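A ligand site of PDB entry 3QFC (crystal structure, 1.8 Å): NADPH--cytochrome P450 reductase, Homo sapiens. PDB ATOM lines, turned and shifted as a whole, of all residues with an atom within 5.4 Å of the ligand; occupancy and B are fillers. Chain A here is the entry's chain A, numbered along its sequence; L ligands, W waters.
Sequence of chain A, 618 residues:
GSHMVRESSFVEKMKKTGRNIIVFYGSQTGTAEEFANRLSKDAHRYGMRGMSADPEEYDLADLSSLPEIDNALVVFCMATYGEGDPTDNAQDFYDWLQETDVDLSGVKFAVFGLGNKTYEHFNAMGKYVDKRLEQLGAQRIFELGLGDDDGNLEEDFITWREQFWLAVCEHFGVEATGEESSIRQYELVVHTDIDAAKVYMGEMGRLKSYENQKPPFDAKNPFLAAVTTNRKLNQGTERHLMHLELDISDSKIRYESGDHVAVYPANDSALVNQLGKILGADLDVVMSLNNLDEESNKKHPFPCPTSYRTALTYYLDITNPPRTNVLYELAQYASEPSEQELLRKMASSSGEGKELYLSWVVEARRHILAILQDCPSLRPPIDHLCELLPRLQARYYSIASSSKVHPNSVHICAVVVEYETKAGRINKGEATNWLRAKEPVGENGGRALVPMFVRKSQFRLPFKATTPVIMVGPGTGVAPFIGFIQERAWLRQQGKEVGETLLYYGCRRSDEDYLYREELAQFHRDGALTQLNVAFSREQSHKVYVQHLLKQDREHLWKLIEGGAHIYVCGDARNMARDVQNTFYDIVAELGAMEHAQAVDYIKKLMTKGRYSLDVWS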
ATOM      1  N   ARG A 239      -3.802  40.177  -3.741  1.00  0.00           N
ATOM      2  CA  ARG A 239      -4.678  39.318  -2.979  1.00  0.00           C
ATOM      3  C   ARG A 239      -5.121  40.169  -1.804  1.00  0.00           C
ATOM      4  O   ARG A 239      -4.584  41.258  -1.574  1.00  0.00           O
ATOM      5  CB  ARG A 239      -3.912  38.109  -2.461  1.00  0.00           C
ATOM      6  CG  ARG A 239      -3.156  37.337  -3.528  1.00  0.00           C
ATOM      7  CD  ARG A 239      -2.706  35.986  -2.982  1.00  0.00           C
ATOM      8  NE  ARG A 239      -1.750  36.121  -1.896  1.00  0.00           N
ATOM      9  CZ  ARG A 239      -1.526  35.177  -0.986  1.00  0.00           C
ATOM     10  NH1 ARG A 239      -2.200  34.023  -1.046  1.00  0.00           N
ATOM     11  NH2 ARG A 239      -0.620  35.357  -0.031  1.00  0.00           N
ATOM     12  N   LEU A 241      -5.634  39.890   2.279  1.00  0.00           N
ATOM     13  CA  LEU A 241      -5.542  39.131   3.519  1.00  0.00           C
ATOM     14  C   LEU A 241      -6.028  40.105   4.570  1.00  0.00           C
ATOM     15  O   LEU A 241      -5.650  41.278   4.563  1.00  0.00           O
ATOM     16  CB  LEU A 241      -4.099  38.675   3.762  1.00  0.00           C
ATOM     17  CG  LEU A 241      -3.768  37.509   2.824  1.00  0.00           C
ATOM     18  CD1 LEU A 241      -2.808  37.982   1.740  1.00  0.00           C
ATOM     19  CD2 LEU A 241      -3.174  36.353   3.623  1.00  0.00           C
ATOM     20  N   VAL A 415      -7.738  34.847   4.198  1.00  0.00           N
ATOM     21  CA  VAL A 415      -7.371  35.273   2.854  1.00  0.00           C
ATOM     22  C   VAL A 415      -8.647  35.191   2.010  1.00  0.00           C
ATOM     23  O   VAL A 415      -9.364  34.177   2.039  1.00  0.00           O
ATOM     24  CB  VAL A 415      -6.282  34.353   2.239  1.00  0.00           C
ATOM     25  CG1 VAL A 415      -6.736  32.896   2.253  1.00  0.00           C
ATOM     26  CG2 VAL A 415      -5.969  34.805   0.828  1.00  0.00           C
ATOM     27  N   PRO A 474       2.680  28.362   7.828  1.00  0.00           N
ATOM     28  CA  PRO A 474       2.890  29.329   6.752  1.00  0.00           C
ATOM     29  C   PRO A 474       1.564  29.929   6.273  1.00  0.00           C
ATOM     30  O   PRO A 474       0.514  29.286   6.377  1.00  0.00           O
ATOM     31  CB  PRO A 474       3.612  28.510   5.691  1.00  0.00           C
ATOM     32  CG  PRO A 474       3.086  27.146   5.869  1.00  0.00           C
ATOM     33  CD  PRO A 474       3.015  26.993   7.382  1.00  0.00           C
ATOM     34  N   GLY A 475       1.604  31.157   5.764  1.00  0.00           N
ATOM     35  CA  GLY A 475       0.393  31.803   5.276  1.00  0.00           C
ATOM     36  C   GLY A 475      -0.650  31.983   6.370  1.00  0.00           C
ATOM     37  O   GLY A 475      -0.307  32.280   7.512  1.00  0.00           O
ATOM     38  N   THR A 476      -1.925  31.791   6.038  1.00  0.00           N
ATOM     39  CA  THR A 476      -2.975  31.943   7.032  1.00  0.00           C
ATOM     40  C   THR A 476      -2.883  30.871   8.120  1.00  0.00           C
ATOM     41  O   THR A 476      -3.590  30.928   9.128  1.00  0.00           O
ATOM     42  CB  THR A 476      -4.389  31.904   6.379  1.00  0.00           C
ATOM     43  OG1 THR A 476      -4.490  30.778   5.502  1.00  0.00           O
ATOM     44  CG2 THR A 476      -4.619  33.197   5.599  1.00  0.00           C
ATOM     45  N   GLY A 477      -2.004  29.895   7.913  1.00  0.00           N
ATOM     46  CA  GLY A 477      -1.821  28.877   8.913  1.00  0.00           C
ATOM     47  C   GLY A 477      -1.214  29.499  10.172  1.00  0.00           C
ATOM     48  O   GLY A 477      -1.132  28.853  11.212  1.00  0.00           O
ATOM     49  N   GLY A 506       5.815  31.366   7.005  1.00  0.00           N
ATOM     50  CA  GLY A 506       6.253  31.558   5.640  1.00  0.00           C
ATOM     51  C   GLY A 506       5.267  32.366   4.823  1.00  0.00           C
ATOM     52  O   GLY A 506       4.065  32.377   5.095  1.00  0.00           O
ATOM     53  N   CYS A 507       5.791  33.064   3.810  1.00  0.00           N
ATOM     54  CA  CYS A 507       4.959  33.857   2.903  1.00  0.00           C
ATOM     55  C   CYS A 507       5.707  33.950   1.584  1.00  0.00           C
ATOM     56  O   CYS A 507       6.886  33.579   1.493  1.00  0.00           O
ATOM     57  CB  CYS A 507       4.670  35.257   3.486  1.00  0.00           C
ATOM     58  SG  CYS A 507       6.089  36.330   3.744  1.00  0.00           S
ATOM     59  N   ARG A 508       5.026  34.423   0.541  1.00  0.00           N
ATOM     60  CA  ARG A 508       5.625  34.529  -0.786  1.00  0.00           C
ATOM     61  C   ARG A 508       6.776  35.532  -0.861  1.00  0.00           C
ATOM     62  O   ARG A 508       7.885  35.187  -1.275  1.00  0.00           O
ATOM     63  CB  ARG A 508       4.538  34.869  -1.808  1.00  0.00           C
ATOM     64  CG  ARG A 508       3.429  33.834  -1.815  1.00  0.00           C
ATOM     65  CD  ARG A 508       2.308  34.156  -2.790  1.00  0.00           C
ATOM     66  NE  ARG A 508       1.196  33.221  -2.586  1.00  0.00           N
ATOM     67  CZ  ARG A 508       0.100  33.195  -3.335  1.00  0.00           C
ATOM     68  NH1 ARG A 508      -0.047  34.046  -4.338  1.00  0.00           N
ATOM     69  NH2 ARG A 508      -0.869  32.333  -3.053  1.00  0.00           N
ATOM     70  N   ASP A 513       3.145  39.825   1.331  1.00  0.00           N
ATOM     71  CA  ASP A 513       2.187  39.094   2.150  1.00  0.00           C
ATOM     72  C   ASP A 513       2.685  38.569   3.495  1.00  0.00           C
ATOM     73  O   ASP A 513       2.301  37.478   3.919  1.00  0.00           O
ATOM     74  CB  ASP A 513       1.589  37.957   1.316  1.00  0.00           C
ATOM     75  CG  ASP A 513       2.632  36.957   0.856  1.00  0.00           C
ATOM     76  OD1 ASP A 513       3.786  37.355   0.654  1.00  0.00           O
ATOM     77  OD2 ASP A 513       2.283  35.766   0.681  1.00  0.00           O
ATOM     78  N   ALA A 535      10.308  31.783   6.142  1.00  0.00           N
ATOM     79  CA  ALA A 535      10.718  31.360   4.818  1.00  0.00           C
ATOM     80  C   ALA A 535       9.974  32.130   3.747  1.00  0.00           C
ATOM     81  O   ALA A 535       8.745  32.049   3.657  1.00  0.00           O
ATOM     82  CB  ALA A 535      10.452  29.871   4.658  1.00  0.00           C
ATOM     83  N   SER A 537       9.191  32.196   0.167  1.00  0.00           N
ATOM     84  CA  SER A 537       9.170  31.253  -0.942  1.00  0.00           C
ATOM     85  C   SER A 537       9.476  31.741  -2.347  1.00  0.00           C
ATOM     86  O   SER A 537       9.957  30.967  -3.174  1.00  0.00           O
ATOM     87  CB  SER A 537       7.827  30.516  -0.959  1.00  0.00           C
ATOM     88  OG  SER A 537       6.765  31.420  -1.186  1.00  0.00           O
ATOM     89  N   ARG A 538       9.205  33.006  -2.640  1.00  0.00           N
ATOM     90  CA  ARG A 538       9.428  33.501  -3.993  1.00  0.00           C
ATOM     91  C   ARG A 538      10.443  34.622  -4.141  1.00  0.00           C
ATOM     92  O   ARG A 538      10.445  35.339  -5.141  1.00  0.00           O
ATOM     93  CB  ARG A 538       8.096  33.951  -4.605  1.00  0.00           C
ATOM     94  CG  ARG A 538       7.032  32.883  -4.568  1.00  0.00           C
ATOM     95  CD  ARG A 538       5.752  33.300  -5.261  1.00  0.00           C
ATOM     96  NE  ARG A 538       4.685  32.341  -5.005  1.00  0.00           N
ATOM     97  CZ  ARG A 538       3.522  32.307  -5.644  1.00  0.00           C
ATOM     98  NH1 ARG A 538       3.264  33.189  -6.591  1.00  0.00           N
ATOM     99  NH2 ARG A 538       2.626  31.382  -5.330  1.00  0.00           N
ATOM    100  N   LYS A 543      12.228  27.386  -4.390  1.00  0.00           N
ATOM    101  CA  LYS A 543      11.317  27.591  -3.268  1.00  0.00           C
ATOM    102  C   LYS A 543      12.059  27.405  -1.949  1.00  0.00           C
ATOM    103  O   LYS A 543      12.908  26.527  -1.826  1.00  0.00           O
ATOM    104  CB  LYS A 543      10.164  26.594  -3.328  1.00  0.00           C
ATOM    105  CG  LYS A 543       9.241  26.740  -4.530  1.00  0.00           C
ATOM    106  CD  LYS A 543       8.461  28.033  -4.491  1.00  0.00           C
ATOM    107  CE  LYS A 543       7.388  28.044  -5.578  1.00  0.00           C
ATOM    108  NZ  LYS A 543       6.652  29.325  -5.629  1.00  0.00           N
ATOM    109  N   TYR A 545      10.823  26.977   1.896  1.00  0.00           N
ATOM    110  CA  TYR A 545       9.640  26.771   2.731  1.00  0.00           C
ATOM    111  C   TYR A 545       9.988  26.551   4.199  1.00  0.00           C
ATOM    112  O   TYR A 545      11.151  26.420   4.564  1.00  0.00           O
ATOM    113  CB  TYR A 545       8.897  25.564   2.215  1.00  0.00           C
ATOM    114  CG  TYR A 545       8.327  25.704   0.807  1.00  0.00           C
ATOM    115  CD1 TYR A 545       8.224  24.593  -0.028  1.00  0.00           C
ATOM    116  CD2 TYR A 545       7.788  26.922   0.372  1.00  0.00           C
ATOM    117  CE1 TYR A 545       7.579  24.678  -1.262  1.00  0.00           C
ATOM    118  CE2 TYR A 545       7.144  27.014  -0.869  1.00  0.00           C
ATOM    119  CZ  TYR A 545       7.038  25.889  -1.676  1.00  0.00           C
ATOM    120  OH  TYR A 545       6.348  25.950  -2.856  1.00  0.00           O
ATOM    121  N   VAL A 546       8.966  26.472   5.041  1.00  0.00           N
ATOM    122  CA  VAL A 546       9.205  26.241   6.467  1.00  0.00           C
ATOM    123  C   VAL A 546       9.957  24.932   6.731  1.00  0.00           C
ATOM    124  O   VAL A 546      10.807  24.882   7.609  1.00  0.00           O
ATOM    125  CB  VAL A 546       7.861  26.241   7.269  1.00  0.00           C
ATOM    126  CG1 VAL A 546       7.322  27.660   7.342  1.00  0.00           C
ATOM    127  CG2 VAL A 546       6.842  25.327   6.607  1.00  0.00           C
ATOM    128  N   GLN A 547       9.674  23.873   5.963  1.00  0.00           N
ATOM    129  CA  GLN A 547      10.382  22.617   6.203  1.00  0.00           C
ATOM    130  C   GLN A 547      11.886  22.742   5.954  1.00  0.00           C
ATOM    131  O   GLN A 547      12.690  22.027   6.582  1.00  0.00           O
ATOM    132  CB  GLN A 547       9.800  21.443   5.377  1.00  0.00           C
ATOM    133  CG  GLN A 547       9.707  21.668   3.868  1.00  0.00           C
ATOM    134  CD  GLN A 547       8.403  22.337   3.460  1.00  0.00           C
ATOM    135  OE1 GLN A 547       7.873  23.178   4.191  1.00  0.00           O
ATOM    136  NE2 GLN A 547       7.884  21.971   2.294  1.00  0.00           N
ATOM    137  N   ASP A 572      -2.210  24.689   5.082  1.00  0.00           N
ATOM    138  CA  ASP A 572      -2.454  23.808   3.932  1.00  0.00           C
ATOM    139  C   ASP A 572      -2.295  22.326   4.250  1.00  0.00           C
ATOM    140  O   ASP A 572      -1.210  21.868   4.607  1.00  0.00           O
ATOM    141  CB  ASP A 572      -1.520  24.162   2.769  1.00  0.00           C
ATOM    142  CG  ASP A 572      -1.678  23.224   1.589  1.00  0.00           C
ATOM    143  OD1 ASP A 572      -0.665  22.660   1.115  1.00  0.00           O
ATOM    144  OD2 ASP A 572      -2.824  23.040   1.130  1.00  0.00           O
ATOM    145  N   ASN A 575      -0.422  19.774   0.747  1.00  0.00           N
ATOM    146  CA  ASN A 575       1.002  19.501   0.561  1.00  0.00           C
ATOM    147  C   ASN A 575       1.897  19.904   1.719  1.00  0.00           C
ATOM    148  O   ASN A 575       2.771  19.146   2.118  1.00  0.00           O
ATOM    149  CB  ASN A 575       1.499  20.185  -0.708  1.00  0.00           C
ATOM    150  CG  ASN A 575       0.912  19.569  -1.959  1.00  0.00           C
ATOM    151  OD1 ASN A 575       0.179  20.220  -2.696  1.00  0.00           O
ATOM    152  ND2 ASN A 575       1.225  18.311  -2.202  1.00  0.00           N
ATOM    153  N   MET A 576       1.680  21.085   2.280  1.00  0.00           N
ATOM    154  CA  MET A 576       2.514  21.564   3.377  1.00  0.00           C
ATOM    155  C   MET A 576       2.552  20.625   4.573  1.00  0.00           C
ATOM    156  O   MET A 576       3.637  20.246   5.036  1.00  0.00           O
ATOM    157  CB  MET A 576       2.053  22.965   3.808  1.00  0.00           C
ATOM    158  CG  MET A 576       2.882  23.615   4.916  1.00  0.00           C
ATOM    159  SD  MET A 576       2.497  23.094   6.601  1.00  0.00           S
ATOM    160  CE  MET A 576       0.837  23.878   6.788  1.00  0.00           C
ATOM    161  N   ASP A 579       4.616  17.556   3.729  1.00  0.00           N
ATOM    162  CA  ASP A 579       6.032  17.874   3.572  1.00  0.00           C
ATOM    163  C   ASP A 579       6.682  18.144   4.930  1.00  0.00           C
ATOM    164  O   ASP A 579       7.830  17.758   5.170  1.00  0.00           O
ATOM    165  CB  ASP A 579       6.214  19.093   2.668  1.00  0.00           C
ATOM    166  CG  ASP A 579       5.899  18.799   1.223  1.00  0.00           C
ATOM    167  OD1 ASP A 579       5.740  19.759   0.437  1.00  0.00           O
ATOM    168  OD2 ASP A 579       5.822  17.603   0.858  1.00  0.00           O
HETATM  169  P1  LIG L   1      -0.163  30.769   0.569  1.00  0.00           P
HETATM  170  O1  LIG L   1       0.323  32.135   0.204  1.00  0.00           O
HETATM  171  O2  LIG L   1      -0.782  30.000  -0.540  1.00  0.00           O
HETATM  172  O3  LIG L   1       1.018  30.012   1.056  1.00  0.00           O
HETATM  173  C1  LIG L   1       1.757  30.280   2.256  1.00  0.00           C
HETATM  174  C2  LIG L   1       3.213  29.912   2.067  1.00  0.00           C
HETATM  175  O4  LIG L   1       3.282  28.471   1.933  1.00  0.00           O
HETATM  176  C3  LIG L   1       3.823  30.486   0.763  1.00  0.00           C
HETATM  177  O5  LIG L   1       5.104  31.103   0.962  1.00  0.00           O
HETATM  178  C4  LIG L   1       3.888  29.288  -0.147  1.00  0.00           C
HETATM  179  O6  LIG L   1       4.871  29.369  -1.204  1.00  0.00           O
HETATM  180  C5  LIG L   1       4.162  28.191   0.874  1.00  0.00           C
HETATM  181  N1  LIG L   1       3.984  26.912   0.398  1.00  0.00           N
HETATM  182  C6  LIG L   1       3.353  26.336  -0.721  1.00  0.00           C
HETATM  183  N2  LIG L   1       3.353  24.979  -0.938  1.00  0.00           N
HETATM  184  C7  LIG L   1       4.071  24.631   0.204  1.00  0.00           C
HETATM  185  C8  LIG L   1       4.507  23.331   0.713  1.00  0.00           C
HETATM  186  N3  LIG L   1       4.241  22.207   0.081  1.00  0.00           N
HETATM  187  N4  LIG L   1       5.197  23.234   1.858  1.00  0.00           N
HETATM  188  C9  LIG L   1       5.534  24.331   2.614  1.00  0.00           C
HETATM  189  N5  LIG L   1       5.226  25.606   2.283  1.00  0.00           N
HETATM  190  C10 LIG L   1       4.451  25.795   1.019  1.00  0.00           C
HETATM  191  O7  LIG L   1      -0.987  30.802   1.818  1.00  0.00           O
HETATM  192  P2  LIG L   1      -2.419  31.388   1.928  1.00  0.00           P
HETATM  193  O8  LIG L   1      -3.185  30.464   1.039  1.00  0.00           O
HETATM  194  O9  LIG L   1      -2.563  32.745   1.322  1.00  0.00           O
HETATM  195  O10 LIG L   1      -2.877  31.347   3.355  1.00  0.00           O
HETATM  196  P3  LIG L   1       4.542  29.380  -2.788  1.00  0.00           P
HETATM  197  O11 LIG L   1       3.061  29.989  -3.028  1.00  0.00           O
HETATM  198  O12 LIG L   1       4.621  27.899  -3.339  1.00  0.00           O
HETATM  199  O13 LIG L   1       5.621  30.329  -3.447  1.00  0.00           O
HETATM  200  O   HOH W   1       6.581  27.682   4.006  1.00  0.00           O
HETATM  201  O   HOH W   2       1.238  26.559   2.634  1.00  0.00           O
HETATM  202  O   HOH W   3      -0.871  27.017   0.157  1.00  0.00           O
HETATM  203  O   HOH W   4       3.500  21.741  -2.958  1.00  0.00           O
HETATM  204  O   HOH W   5       0.739  28.520  -2.554  1.00  0.00           O
HETATM  205  O   HOH W   6       1.912  33.572   1.941  1.00  0.00           O
HETATM  206  O   HOH W   7       7.021  30.068   2.719  1.00  0.00           O
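Pro 474 touches the ligand (CB to O4, 3.8 Å). Gly 475 touches the ligand (N to C1, 3.6 Å). Gly 506 touches the ligand (O to C2, 3.996 Å). Asn 575 touches the ligand. CA of Met 576 touches N4 of the ligand, 3.5 Å away. Within 4 Å of the ligand: Arg 239, Pro 474, Gly 475, Thr 476, Gly 506, Cys 507, Arg 508, Ser 537, Arg 538, Lys 543, Tyr 545, Gln 547, Asn 575, Met 576 and Asp 579. The nearest printed residue that does not touch the ligand is Val 415 (4.01 Å).
Water W6 bridges OD2 of Asp 513 (2.6 Å) and O1 of the ligand (2.8 Å). Water W7 lies within hydrogen-bond range of the backbone carbonyl oxygen of Ala 535 (2.8 Å), an oxygen (O5) of the ligand (2.8 Å) and the backbone NH of Cys 507 (3.4 Å). Water W1 lies within hydrogen-bond range of N of Val 546 (2.9 Å) and N5 of the ligand (3.0 Å).
O13 of the ligand lies within salt-bridge range of NZ of Lys 543, 2.6 Å away. OH of Tyr 545 sits at hydrogen-bond distance from O12 of the ligand (2.6 Å). An oxygen (O13) of the ligand is in salt-bridge range of the guanidinium group (NE) of Arg 538. The guanidinium group (NH1) of Arg 239 is in salt-bridge range of an oxygen (O9) of the ligand, 2.7 Å away. OG of Ser 537 lies within hydrogen-bond range of O5 of the ligand (2.7 Å). The backbone NH of Thr 476 sits at hydrogen-bond distance from an oxygen (O10) of the ligand, 2.9 Å away. An oxygen (O10) of the ligand lies within hydrogen-bond range of the side-chain hydroxyl (OG1) of Thr 476 (2.7 Å). The side-chain carboxylate of Asp 579 is in hydrogen-bond range of a nitrogen (N3) of the ligand (2.9 Å). O of Cys 507 sits close to O5 of the ligand (3.1 Å). The side-chain amide nitrogen of Gln 547 lies within hydrogen-bond range of a nitrogen (N4) of the ligand, at 3.0 Å. An oxygen (O5) of the ligand is in hydrogen-bond range of the backbone NH of Arg 508 (3.3 Å). NE of Arg 508 lies within salt-bridge range of O1 of the ligand (3.1 Å).
The backbone carbonyl oxygen (O) of Arg 508 lies within hydrogen-bond range of the backbone NH (N) of Arg 538, 2.9 Å away. The guanidinium group (NH2) of Arg 239 lies within salt-bridge range of the side-chain carboxylate (OD2) of Asp 513, at 3.0 Å. The backbone carbonyl oxygen of Cys 507 lies within hydrogen-bond range of the backbone NH of Ser 537 (3.0 Å). The backbone NH of Cys 507 is in hydrogen-bond range of the backbone carbonyl oxygen of Ala 535 (3.1 Å). The side-chain carboxylate (OD2) of Asp 513 lies within hydrogen-bond range of the backbone NH (N) of Arg 508 (3.1 Å). N of Asn 575 sits at hydrogen-bond distance from OD1 of Asp 572 (2.9 Å). The side-chain carboxylate of Asp 572 sits at hydrogen-bond distance from the backbone NH of Met 576, at 3.1 Å. N of Gly 475 is in hydrogen-bond range of O of Gly 506, 2.8 Å away.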
